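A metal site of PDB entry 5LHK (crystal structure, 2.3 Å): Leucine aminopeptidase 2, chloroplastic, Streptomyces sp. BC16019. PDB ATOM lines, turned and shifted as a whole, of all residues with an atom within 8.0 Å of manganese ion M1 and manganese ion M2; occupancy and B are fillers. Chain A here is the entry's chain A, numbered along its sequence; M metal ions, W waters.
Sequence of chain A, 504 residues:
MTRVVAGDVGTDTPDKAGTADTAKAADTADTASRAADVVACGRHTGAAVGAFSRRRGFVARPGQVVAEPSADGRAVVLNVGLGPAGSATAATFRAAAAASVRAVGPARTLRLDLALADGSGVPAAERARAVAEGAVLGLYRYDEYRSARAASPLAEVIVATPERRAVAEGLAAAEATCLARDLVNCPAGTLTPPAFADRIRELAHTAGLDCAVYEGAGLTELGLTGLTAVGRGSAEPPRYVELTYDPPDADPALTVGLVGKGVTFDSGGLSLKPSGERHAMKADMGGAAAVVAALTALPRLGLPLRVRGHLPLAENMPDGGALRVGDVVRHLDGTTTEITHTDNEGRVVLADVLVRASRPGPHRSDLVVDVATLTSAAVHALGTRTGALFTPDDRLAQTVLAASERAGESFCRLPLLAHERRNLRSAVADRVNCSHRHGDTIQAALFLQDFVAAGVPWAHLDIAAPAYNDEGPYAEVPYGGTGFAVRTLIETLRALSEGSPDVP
Of the 30 residues printed, 3 come within 4 Å of manganese ion M1. Along chain A the residues within 4 Å of manganese ion M1 span positions 266 to 345.
Manganese ion M1 is bound by the side-chain carboxylate of Asp 266 (2.1 Å), the backbone carbonyl oxygen of Asp 343 (2.2 Å), the side-chain carboxylate of Asp 343 (2.2 Å), the side-chain carboxylate of Glu 345 (2.2 Å), water W3 (2.3 Å) and water W1 (2.6 Å). Manganese ion M1 has six donor atoms within binding distance.
Water W2 bridges the side-chain carboxylate of Asp 284 and the backbone carbonyl oxygen of Thr 373.
The side-chain carboxylate of Glu 345 lies close to the side-chain amide nitrogen of Asn 316, 3.5 Å away. The backbone NH (N) of Asp 343 sits close to a ring nitrogen (ND1) of His 341 (3.3 Å). The side-chain hydroxyl (OG1) of Thr 373 is in hydrogen-bond range of the side-chain carboxylate (OD1) of Asp 284 (2.9 Å). OD2 of Asp 343 is in salt-bridge range of NZ of Lys 273, at 2.8 Å. The backbone NH (N) of Asp 266 lies within hydrogen-bond range of the backbone carbonyl oxygen (O) of Met 281, at 3.1 Å. N of Gly 268 sits at hydrogen-bond distance from OD1 of Asp 266, 3.1 Å away. The side-chain carboxylate (OD1) of Asp 266 lies within hydrogen-bond range of the side-chain amide nitrogen (ND2) of Asn 316, at 3.0 Å. The side-chain amino group (NZ) of Lys 261 sits close to the backbone carbonyl oxygen (O) of Thr 373 (3.0 Å).
OD2 of Asp 284 is bound to manganese ion M2 (2.0 Å). The side-chain carboxylate (OE2) of Glu 345 is bound to manganese ion M2 (2.1 Å). Water W3 is bound to manganese ion M2. OD2 of Asp 266 binds manganese ion M2. Manganese ion M2 is bound by NZ of Lys 261 (2.4 Å). Manganese ion M2 has five donor atoms within binding distance.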
ATOM      1  N   VAL A 230       1.802 -24.720 -17.389  1.00  0.00           N
ATOM      2  CA  VAL A 230       1.163 -23.486 -17.834  1.00  0.00           C
ATOM      3  C   VAL A 230       1.097 -22.425 -16.725  1.00  0.00           C
ATOM      4  O   VAL A 230       1.357 -21.242 -16.982  1.00  0.00           O
ATOM      5  CB  VAL A 230      -0.247 -23.773 -18.410  1.00  0.00           C
ATOM      6  CG1 VAL A 230      -1.064 -22.489 -18.568  1.00  0.00           C
ATOM      7  CG2 VAL A 230      -0.122 -24.496 -19.755  1.00  0.00           C
ATOM      8  N   LYS A 261     -12.441 -25.378 -18.364  1.00  0.00           N
ATOM      9  CA  LYS A 261     -11.183 -24.648 -18.451  1.00  0.00           C
ATOM     10  C   LYS A 261     -11.254 -23.357 -17.623  1.00  0.00           C
ATOM     11  O   LYS A 261     -12.067 -22.480 -17.912  1.00  0.00           O
ATOM     12  CB  LYS A 261     -10.874 -24.298 -19.900  1.00  0.00           C
ATOM     13  CG  LYS A 261      -9.604 -23.456 -20.089  1.00  0.00           C
ATOM     14  CD  LYS A 261      -9.522 -22.904 -21.485  1.00  0.00           C
ATOM     15  CE  LYS A 261      -8.375 -21.909 -21.599  1.00  0.00           C
ATOM     16  NZ  LYS A 261      -8.262 -21.433 -23.002  1.00  0.00           N
ATOM     17  N   GLY A 262     -10.401 -23.259 -16.610  1.00  0.00           N
ATOM     18  CA  GLY A 262     -10.377 -22.127 -15.690  1.00  0.00           C
ATOM     19  C   GLY A 262      -9.103 -21.303 -15.724  1.00  0.00           C
ATOM     20  O   GLY A 262      -8.479 -21.056 -14.694  1.00  0.00           O
ATOM     21  N   VAL A 263      -8.702 -20.854 -16.893  1.00  0.00           N
ATOM     22  CA  VAL A 263      -7.560 -19.942 -16.985  1.00  0.00           C
ATOM     23  C   VAL A 263      -8.099 -18.568 -16.583  1.00  0.00           C
ATOM     24  O   VAL A 263      -8.832 -17.931 -17.334  1.00  0.00           O
ATOM     25  CB  VAL A 263      -6.910 -19.942 -18.386  1.00  0.00           C
ATOM     26  CG1 VAL A 263      -5.796 -18.915 -18.460  1.00  0.00           C
ATOM     27  CG2 VAL A 263      -6.370 -21.332 -18.707  1.00  0.00           C
ATOM     28  N   THR A 264      -7.753 -18.149 -15.376  1.00  0.00           N
ATOM     29  CA  THR A 264      -8.316 -16.945 -14.799  1.00  0.00           C
ATOM     30  C   THR A 264      -7.788 -15.695 -15.476  1.00  0.00           C
ATOM     31  O   THR A 264      -8.443 -14.664 -15.446  1.00  0.00           O
ATOM     32  CB  THR A 264      -8.078 -16.865 -13.289  1.00  0.00           C
ATOM     33  OG1 THR A 264      -6.673 -16.887 -13.019  1.00  0.00           O
ATOM     34  CG2 THR A 264      -8.775 -18.035 -12.607  1.00  0.00           C
ATOM     35  N   PHE A 265      -6.602 -15.789 -16.077  1.00  0.00           N
ATOM     36  CA  PHE A 265      -6.038 -14.717 -16.876  1.00  0.00           C
ATOM     37  C   PHE A 265      -5.105 -15.312 -17.916  1.00  0.00           C
ATOM     38  O   PHE A 265      -4.099 -15.929 -17.568  1.00  0.00           O
ATOM     39  CB  PHE A 265      -5.267 -13.745 -15.991  1.00  0.00           C
ATOM     40  CG  PHE A 265      -4.761 -12.534 -16.727  1.00  0.00           C
ATOM     41  CD1 PHE A 265      -5.655 -11.573 -17.196  1.00  0.00           C
ATOM     42  CD2 PHE A 265      -3.406 -12.382 -16.985  1.00  0.00           C
ATOM     43  CE1 PHE A 265      -5.189 -10.465 -17.905  1.00  0.00           C
ATOM     44  CE2 PHE A 265      -2.936 -11.286 -17.688  1.00  0.00           C
ATOM     45  CZ  PHE A 265      -3.829 -10.318 -18.145  1.00  0.00           C
ATOM     46  N   ASP A 266      -5.448 -15.109 -19.182  1.00  0.00           N
ATOM     47  CA  ASP A 266      -4.625 -15.588 -20.289  1.00  0.00           C
ATOM     48  C   ASP A 266      -3.918 -14.438 -21.000  1.00  0.00           C
ATOM     49  O   ASP A 266      -4.468 -13.855 -21.923  1.00  0.00           O
ATOM     50  CB  ASP A 266      -5.492 -16.399 -21.265  1.00  0.00           C
ATOM     51  CG  ASP A 266      -4.674 -17.122 -22.318  1.00  0.00           C
ATOM     52  OD1 ASP A 266      -3.416 -17.128 -22.228  1.00  0.00           O
ATOM     53  OD2 ASP A 266      -5.289 -17.702 -23.248  1.00  0.00           O
ATOM     54  N   SER A 267      -2.691 -14.138 -20.583  1.00  0.00           N
ATOM     55  CA  SER A 267      -1.869 -13.153 -21.274  1.00  0.00           C
ATOM     56  C   SER A 267      -1.246 -13.656 -22.568  1.00  0.00           C
ATOM     57  O   SER A 267      -0.771 -12.871 -23.367  1.00  0.00           O
ATOM     58  CB  SER A 267      -0.727 -12.671 -20.388  1.00  0.00           C
ATOM     59  OG  SER A 267       0.304 -13.648 -20.368  1.00  0.00           O
ATOM     60  N   GLY A 268      -1.202 -14.972 -22.721  1.00  0.00           N
ATOM     61  CA  GLY A 268      -0.477 -15.610 -23.801  1.00  0.00           C
ATOM     62  C   GLY A 268       0.770 -16.336 -23.355  1.00  0.00           C
ATOM     63  O   GLY A 268       1.212 -17.256 -24.025  1.00  0.00           O
ATOM     64  N   GLY A 269       1.319 -15.929 -22.207  1.00  0.00           N
ATOM     65  CA  GLY A 269       2.601 -16.429 -21.743  1.00  0.00           C
ATOM     66  C   GLY A 269       3.736 -15.733 -22.491  1.00  0.00           C
ATOM     67  O   GLY A 269       3.611 -14.561 -22.837  1.00  0.00           O
ATOM     68  N   SER A 271       4.689 -16.348 -25.514  1.00  0.00           N
ATOM     69  CA  SER A 271       4.017 -16.018 -26.762  1.00  0.00           C
ATOM     70  C   SER A 271       2.921 -15.009 -26.433  1.00  0.00           C
ATOM     71  O   SER A 271       1.696 -15.286 -26.491  1.00  0.00           O
ATOM     72  CB  SER A 271       3.434 -17.277 -27.433  1.00  0.00           C
ATOM     73  OG  SER A 271       4.399 -18.335 -27.535  1.00  0.00           O
ATOM     74  N   LYS A 273       0.300 -12.100 -26.018  1.00  0.00           N
ATOM     75  CA  LYS A 273      -0.751 -11.557 -26.856  1.00  0.00           C
ATOM     76  C   LYS A 273      -0.367 -10.135 -27.265  1.00  0.00           C
ATOM     77  O   LYS A 273       0.084  -9.370 -26.423  1.00  0.00           O
ATOM     78  CB  LYS A 273      -2.102 -11.548 -26.137  1.00  0.00           C
ATOM     79  CG  LYS A 273      -2.724 -12.923 -26.057  1.00  0.00           C
ATOM     80  CD  LYS A 273      -3.998 -12.922 -25.232  1.00  0.00           C
ATOM     81  CE  LYS A 273      -4.501 -14.338 -24.982  1.00  0.00           C
ATOM     82  NZ  LYS A 273      -4.952 -14.980 -26.231  1.00  0.00           N
ATOM     83  N   MET A 281      -8.944 -11.064 -21.584  1.00  0.00           N
ATOM     84  CA  MET A 281      -8.009 -12.056 -21.059  1.00  0.00           C
ATOM     85  C   MET A 281      -8.503 -12.663 -19.736  1.00  0.00           C
ATOM     86  O   MET A 281      -8.246 -13.835 -19.469  1.00  0.00           O
ATOM     87  CB  MET A 281      -6.594 -11.431 -20.886  1.00  0.00           C
ATOM     88  CG  MET A 281      -5.883 -11.151 -22.218  1.00  0.00           C
ATOM     89  SD  MET A 281      -4.728  -9.769 -22.326  1.00  0.00           S
ATOM     90  CE  MET A 281      -3.359 -10.143 -21.305  1.00  0.00           C
ATOM     91  N   ALA A 283     -11.560 -13.391 -19.172  1.00  0.00           N
ATOM     92  CA  ALA A 283     -12.714 -14.228 -19.507  1.00  0.00           C
ATOM     93  C   ALA A 283     -12.349 -15.641 -19.936  1.00  0.00           C
ATOM     94  O   ALA A 283     -13.229 -16.408 -20.338  1.00  0.00           O
ATOM     95  CB  ALA A 283     -13.538 -13.565 -20.623  1.00  0.00           C
ATOM     96  N   ASP A 284     -11.074 -16.020 -19.811  1.00  0.00           N
ATOM     97  CA  ASP A 284     -10.610 -17.297 -20.295  1.00  0.00           C
ATOM     98  C   ASP A 284     -10.948 -18.437 -19.308  1.00  0.00           C
ATOM     99  O   ASP A 284     -10.512 -19.576 -19.478  1.00  0.00           O
ATOM    100  CB  ASP A 284      -9.106 -17.202 -20.578  1.00  0.00           C
ATOM    101  CG  ASP A 284      -8.640 -18.202 -21.609  1.00  0.00           C
ATOM    102  OD1 ASP A 284      -9.409 -18.509 -22.551  1.00  0.00           O
ATOM    103  OD2 ASP A 284      -7.479 -18.675 -21.500  1.00  0.00           O
ATOM    104  N   MET A 285     -11.738 -18.130 -18.277  1.00  0.00           N
ATOM    105  CA  MET A 285     -12.239 -19.115 -17.311  1.00  0.00           C
ATOM    106  C   MET A 285     -13.755 -19.328 -17.463  1.00  0.00           C
ATOM    107  O   MET A 285     -14.393 -19.879 -16.567  1.00  0.00           O
ATOM    108  CB  MET A 285     -11.841 -18.710 -15.865  1.00  0.00           C
ATOM    109  CG  MET A 285     -11.966 -17.222 -15.504  1.00  0.00           C
ATOM    110  SD  MET A 285     -13.558 -16.448 -15.863  1.00  0.00           S
ATOM    111  CE  MET A 285     -14.596 -17.177 -14.625  1.00  0.00           C
ATOM    112  N   ASN A 316      -1.906 -17.706 -17.099  1.00  0.00           N
ATOM    113  CA  ASN A 316      -0.857 -17.841 -18.122  1.00  0.00           C
ATOM    114  C   ASN A 316      -0.134 -16.503 -18.283  1.00  0.00           C
ATOM    115  O   ASN A 316      -0.666 -15.579 -18.895  1.00  0.00           O
ATOM    116  CB  ASN A 316      -1.474 -18.307 -19.428  1.00  0.00           C
ATOM    117  CG  ASN A 316      -0.440 -18.637 -20.489  1.00  0.00           C
ATOM    118  OD1 ASN A 316       0.748 -18.819 -20.202  1.00  0.00           O
ATOM    119  ND2 ASN A 316      -0.894 -18.702 -21.732  1.00  0.00           N
ATOM    120  N   HIS A 341       3.507 -23.051 -29.171  1.00  0.00           N
ATOM    121  CA  HIS A 341       2.941 -21.725 -28.967  1.00  0.00           C
ATOM    122  C   HIS A 341       2.345 -21.677 -27.546  1.00  0.00           C
ATOM    123  O   HIS A 341       1.418 -22.451 -27.241  1.00  0.00           O
ATOM    124  CB  HIS A 341       1.873 -21.434 -30.030  1.00  0.00           C
ATOM    125  CG  HIS A 341       1.584 -19.982 -30.223  1.00  0.00           C
ATOM    126  ND1 HIS A 341       1.082 -19.183 -29.226  1.00  0.00           N
ATOM    127  CD2 HIS A 341       1.711 -19.178 -31.307  1.00  0.00           C
ATOM    128  CE1 HIS A 341       0.911 -17.955 -29.673  1.00  0.00           C
ATOM    129  NE2 HIS A 341       1.293 -17.918 -30.937  1.00  0.00           N
ATOM    130  N   THR A 342       2.847 -20.779 -26.682  1.00  0.00           N
ATOM    131  CA  THR A 342       2.436 -20.760 -25.277  1.00  0.00           C
ATOM    132  C   THR A 342       0.996 -20.263 -25.055  1.00  0.00           C
ATOM    133  O   THR A 342       0.426 -20.432 -23.968  1.00  0.00           O
ATOM    134  CB  THR A 342       3.404 -19.999 -24.342  1.00  0.00           C
ATOM    135  OG1 THR A 342       3.375 -18.586 -24.607  1.00  0.00           O
ATOM    136  CG2 THR A 342       4.817 -20.504 -24.494  1.00  0.00           C
ATOM    137  N   ASP A 343       0.438 -19.600 -26.062  1.00  0.00           N
ATOM    138  CA  ASP A 343      -0.940 -19.123 -26.034  1.00  0.00           C
ATOM    139  C   ASP A 343      -1.998 -20.186 -26.371  1.00  0.00           C
ATOM    140  O   ASP A 343      -3.193 -19.922 -26.259  1.00  0.00           O
ATOM    141  CB  ASP A 343      -1.127 -17.921 -26.967  1.00  0.00           C
ATOM    142  CG  ASP A 343      -2.283 -17.010 -26.541  1.00  0.00           C
ATOM    143  OD1 ASP A 343      -2.862 -17.209 -25.437  1.00  0.00           O
ATOM    144  OD2 ASP A 343      -2.611 -16.088 -27.306  1.00  0.00           O
ATOM    145  N   ASN A 344      -1.572 -21.382 -26.769  1.00  0.00           N
ATOM    146  CA  ASN A 344      -2.481 -22.530 -26.848  1.00  0.00           C
ATOM    147  C   ASN A 344      -2.338 -23.384 -25.596  1.00  0.00           C
ATOM    148  O   ASN A 344      -2.082 -24.591 -25.649  1.00  0.00           O
ATOM    149  CB  ASN A 344      -2.243 -23.346 -28.131  1.00  0.00           C
ATOM    150  CG  ASN A 344      -2.801 -22.661 -29.368  1.00  0.00           C
ATOM    151  OD1 ASN A 344      -3.250 -21.526 -29.324  1.00  0.00           O
ATOM    152  ND2 ASN A 344      -2.768 -23.357 -30.497  1.00  0.00           N
ATOM    153  N   GLU A 345      -2.549 -22.729 -24.460  1.00  0.00           N
ATOM    154  CA  GLU A 345      -2.302 -23.311 -23.152  1.00  0.00           C
ATOM    155  C   GLU A 345      -3.484 -24.129 -22.649  1.00  0.00           C
ATOM    156  O   GLU A 345      -3.275 -25.099 -21.918  1.00  0.00           O
ATOM    157  CB  GLU A 345      -1.941 -22.215 -22.131  1.00  0.00           C
ATOM    158  CG  GLU A 345      -3.117 -21.492 -21.440  1.00  0.00           C
ATOM    159  CD  GLU A 345      -4.006 -20.683 -22.359  1.00  0.00           C
ATOM    160  OE1 GLU A 345      -3.521 -20.222 -23.409  1.00  0.00           O
ATOM    161  OE2 GLU A 345      -5.198 -20.493 -22.021  1.00  0.00           O
ATOM    162  N   GLY A 346      -4.700 -23.755 -23.016  1.00  0.00           N
ATOM    163  CA  GLY A 346      -5.897 -24.417 -22.477  1.00  0.00           C
ATOM    164  C   GLY A 346      -5.963 -25.912 -22.744  1.00  0.00           C
ATOM    165  O   GLY A 346      -6.328 -26.698 -21.869  1.00  0.00           O
ATOM    166  N   ARG A 347      -5.621 -26.314 -23.976  1.00  0.00           N
ATOM    167  CA  ARG A 347      -5.676 -27.731 -24.343  1.00  0.00           C
ATOM    168  C   ARG A 347      -4.668 -28.553 -23.536  1.00  0.00           C
ATOM    169  O   ARG A 347      -4.945 -29.704 -23.158  1.00  0.00           O
ATOM    170  CB  ARG A 347      -5.485 -27.910 -25.860  1.00  0.00           C
ATOM    171  CG  ARG A 347      -4.080 -27.604 -26.391  1.00  0.00           C
ATOM    172  CD  ARG A 347      -4.066 -27.374 -27.897  1.00  0.00           C
ATOM    173  NE  ARG A 347      -4.751 -26.136 -28.254  1.00  0.00           N
ATOM    174  CZ  ARG A 347      -5.042 -25.718 -29.486  1.00  0.00           C
ATOM    175  NH1 ARG A 347      -4.701 -26.445 -30.548  1.00  0.00           N
ATOM    176  NH2 ARG A 347      -5.686 -24.567 -29.652  1.00  0.00           N
ATOM    177  N   ALA A 372     -14.916 -24.984 -22.655  1.00  0.00           N
ATOM    178  CA  ALA A 372     -13.682 -24.224 -22.716  1.00  0.00           C
ATOM    179  C   ALA A 372     -13.765 -23.049 -23.695  1.00  0.00           C
ATOM    180  O   ALA A 372     -14.227 -23.195 -24.829  1.00  0.00           O
ATOM    181  CB  ALA A 372     -12.547 -25.150 -23.108  1.00  0.00           C
ATOM    182  N   THR A 373     -13.307 -21.882 -23.250  1.00  0.00           N
ATOM    183  CA  THR A 373     -13.020 -20.754 -24.140  1.00  0.00           C
ATOM    184  C   THR A 373     -11.669 -21.035 -24.815  1.00  0.00           C
ATOM    185  O   THR A 373     -10.635 -20.442 -24.469  1.00  0.00           O
ATOM    186  CB  THR A 373     -12.964 -19.446 -23.342  1.00  0.00           C
ATOM    187  OG1 THR A 373     -12.059 -19.589 -22.248  1.00  0.00           O
ATOM    188  CG2 THR A 373     -14.358 -19.102 -22.789  1.00  0.00           C
ATOM    189  N   LEU A 374     -11.677 -21.975 -25.752  1.00  0.00           N
ATOM    190  CA  LEU A 374     -10.415 -22.645 -26.153  1.00  0.00           C
ATOM    191  C   LEU A 374      -9.712 -22.005 -27.343  1.00  0.00           C
ATOM    192  O   LEU A 374      -8.505 -21.804 -27.323  1.00  0.00           O
ATOM    193  CB  LEU A 374     -10.667 -24.131 -26.441  1.00  0.00           C
ATOM    194  CG  LEU A 374      -9.420 -25.024 -26.437  1.00  0.00           C
ATOM    195  CD1 LEU A 374      -8.749 -25.074 -25.060  1.00  0.00           C
ATOM    196  CD2 LEU A 374      -9.782 -26.433 -26.899  1.00  0.00           C
ATOM    197  N   THR A 375     -10.470 -21.645 -28.345  1.00  0.00           N
ATOM    198  CA  THR A 375      -9.901 -21.362 -29.648  1.00  0.00           C
ATOM    199  C   THR A 375     -10.388 -20.013 -30.179  1.00  0.00           C
ATOM    200  O   THR A 375     -11.548 -19.650 -30.017  1.00  0.00           O
ATOM    201  CB  THR A 375     -10.257 -22.555 -30.568  1.00  0.00           C
ATOM    202  OG1 THR A 375      -9.370 -23.653 -30.273  1.00  0.00           O
ATOM    203  CG2 THR A 375     -10.071 -22.248 -31.898  1.00  0.00           C
ATOM    204  N   SER A 376      -9.504 -19.296 -30.830  1.00  0.00           N
ATOM    205  CA  SER A 376      -9.863 -18.040 -31.486  1.00  0.00           C
ATOM    206  C   SER A 376     -10.145 -18.212 -32.976  1.00  0.00           C
ATOM    207  O   SER A 376     -10.623 -17.295 -33.594  1.00  0.00           O
ATOM    208  CB  SER A 376      -8.753 -17.035 -31.297  1.00  0.00           C
ATOM    209  OG  SER A 376      -7.525 -17.642 -31.618  1.00  0.00           O
ATOM    210  N   ALA A 464     -15.329 -19.786 -26.799  1.00  0.00           N
ATOM    211  CA  ALA A 464     -14.494 -18.582 -26.642  1.00  0.00           C
ATOM    212  C   ALA A 464     -15.245 -17.311 -27.013  1.00  0.00           C
ATOM    213  O   ALA A 464     -15.315 -16.384 -26.219  1.00  0.00           O
ATOM    214  CB  ALA A 464     -13.221 -18.699 -27.476  1.00  0.00           C
HETATM  215 MN    MN M   1      -4.296 -18.723 -24.848  1.00  0.00          MN
HETATM  216 MN    MN M   2      -6.708 -19.598 -23.120  1.00  0.00          MN
HETATM  217  O   HOH W   1      -5.624 -17.892 -26.872  1.00  0.00           O
HETATM  218  O   HOH W   2      -8.393 -18.434 -25.245  1.00  0.00           O
HETATM  219  O   HOH W   3      -6.264 -19.889 -25.272  1.00  0.00           O
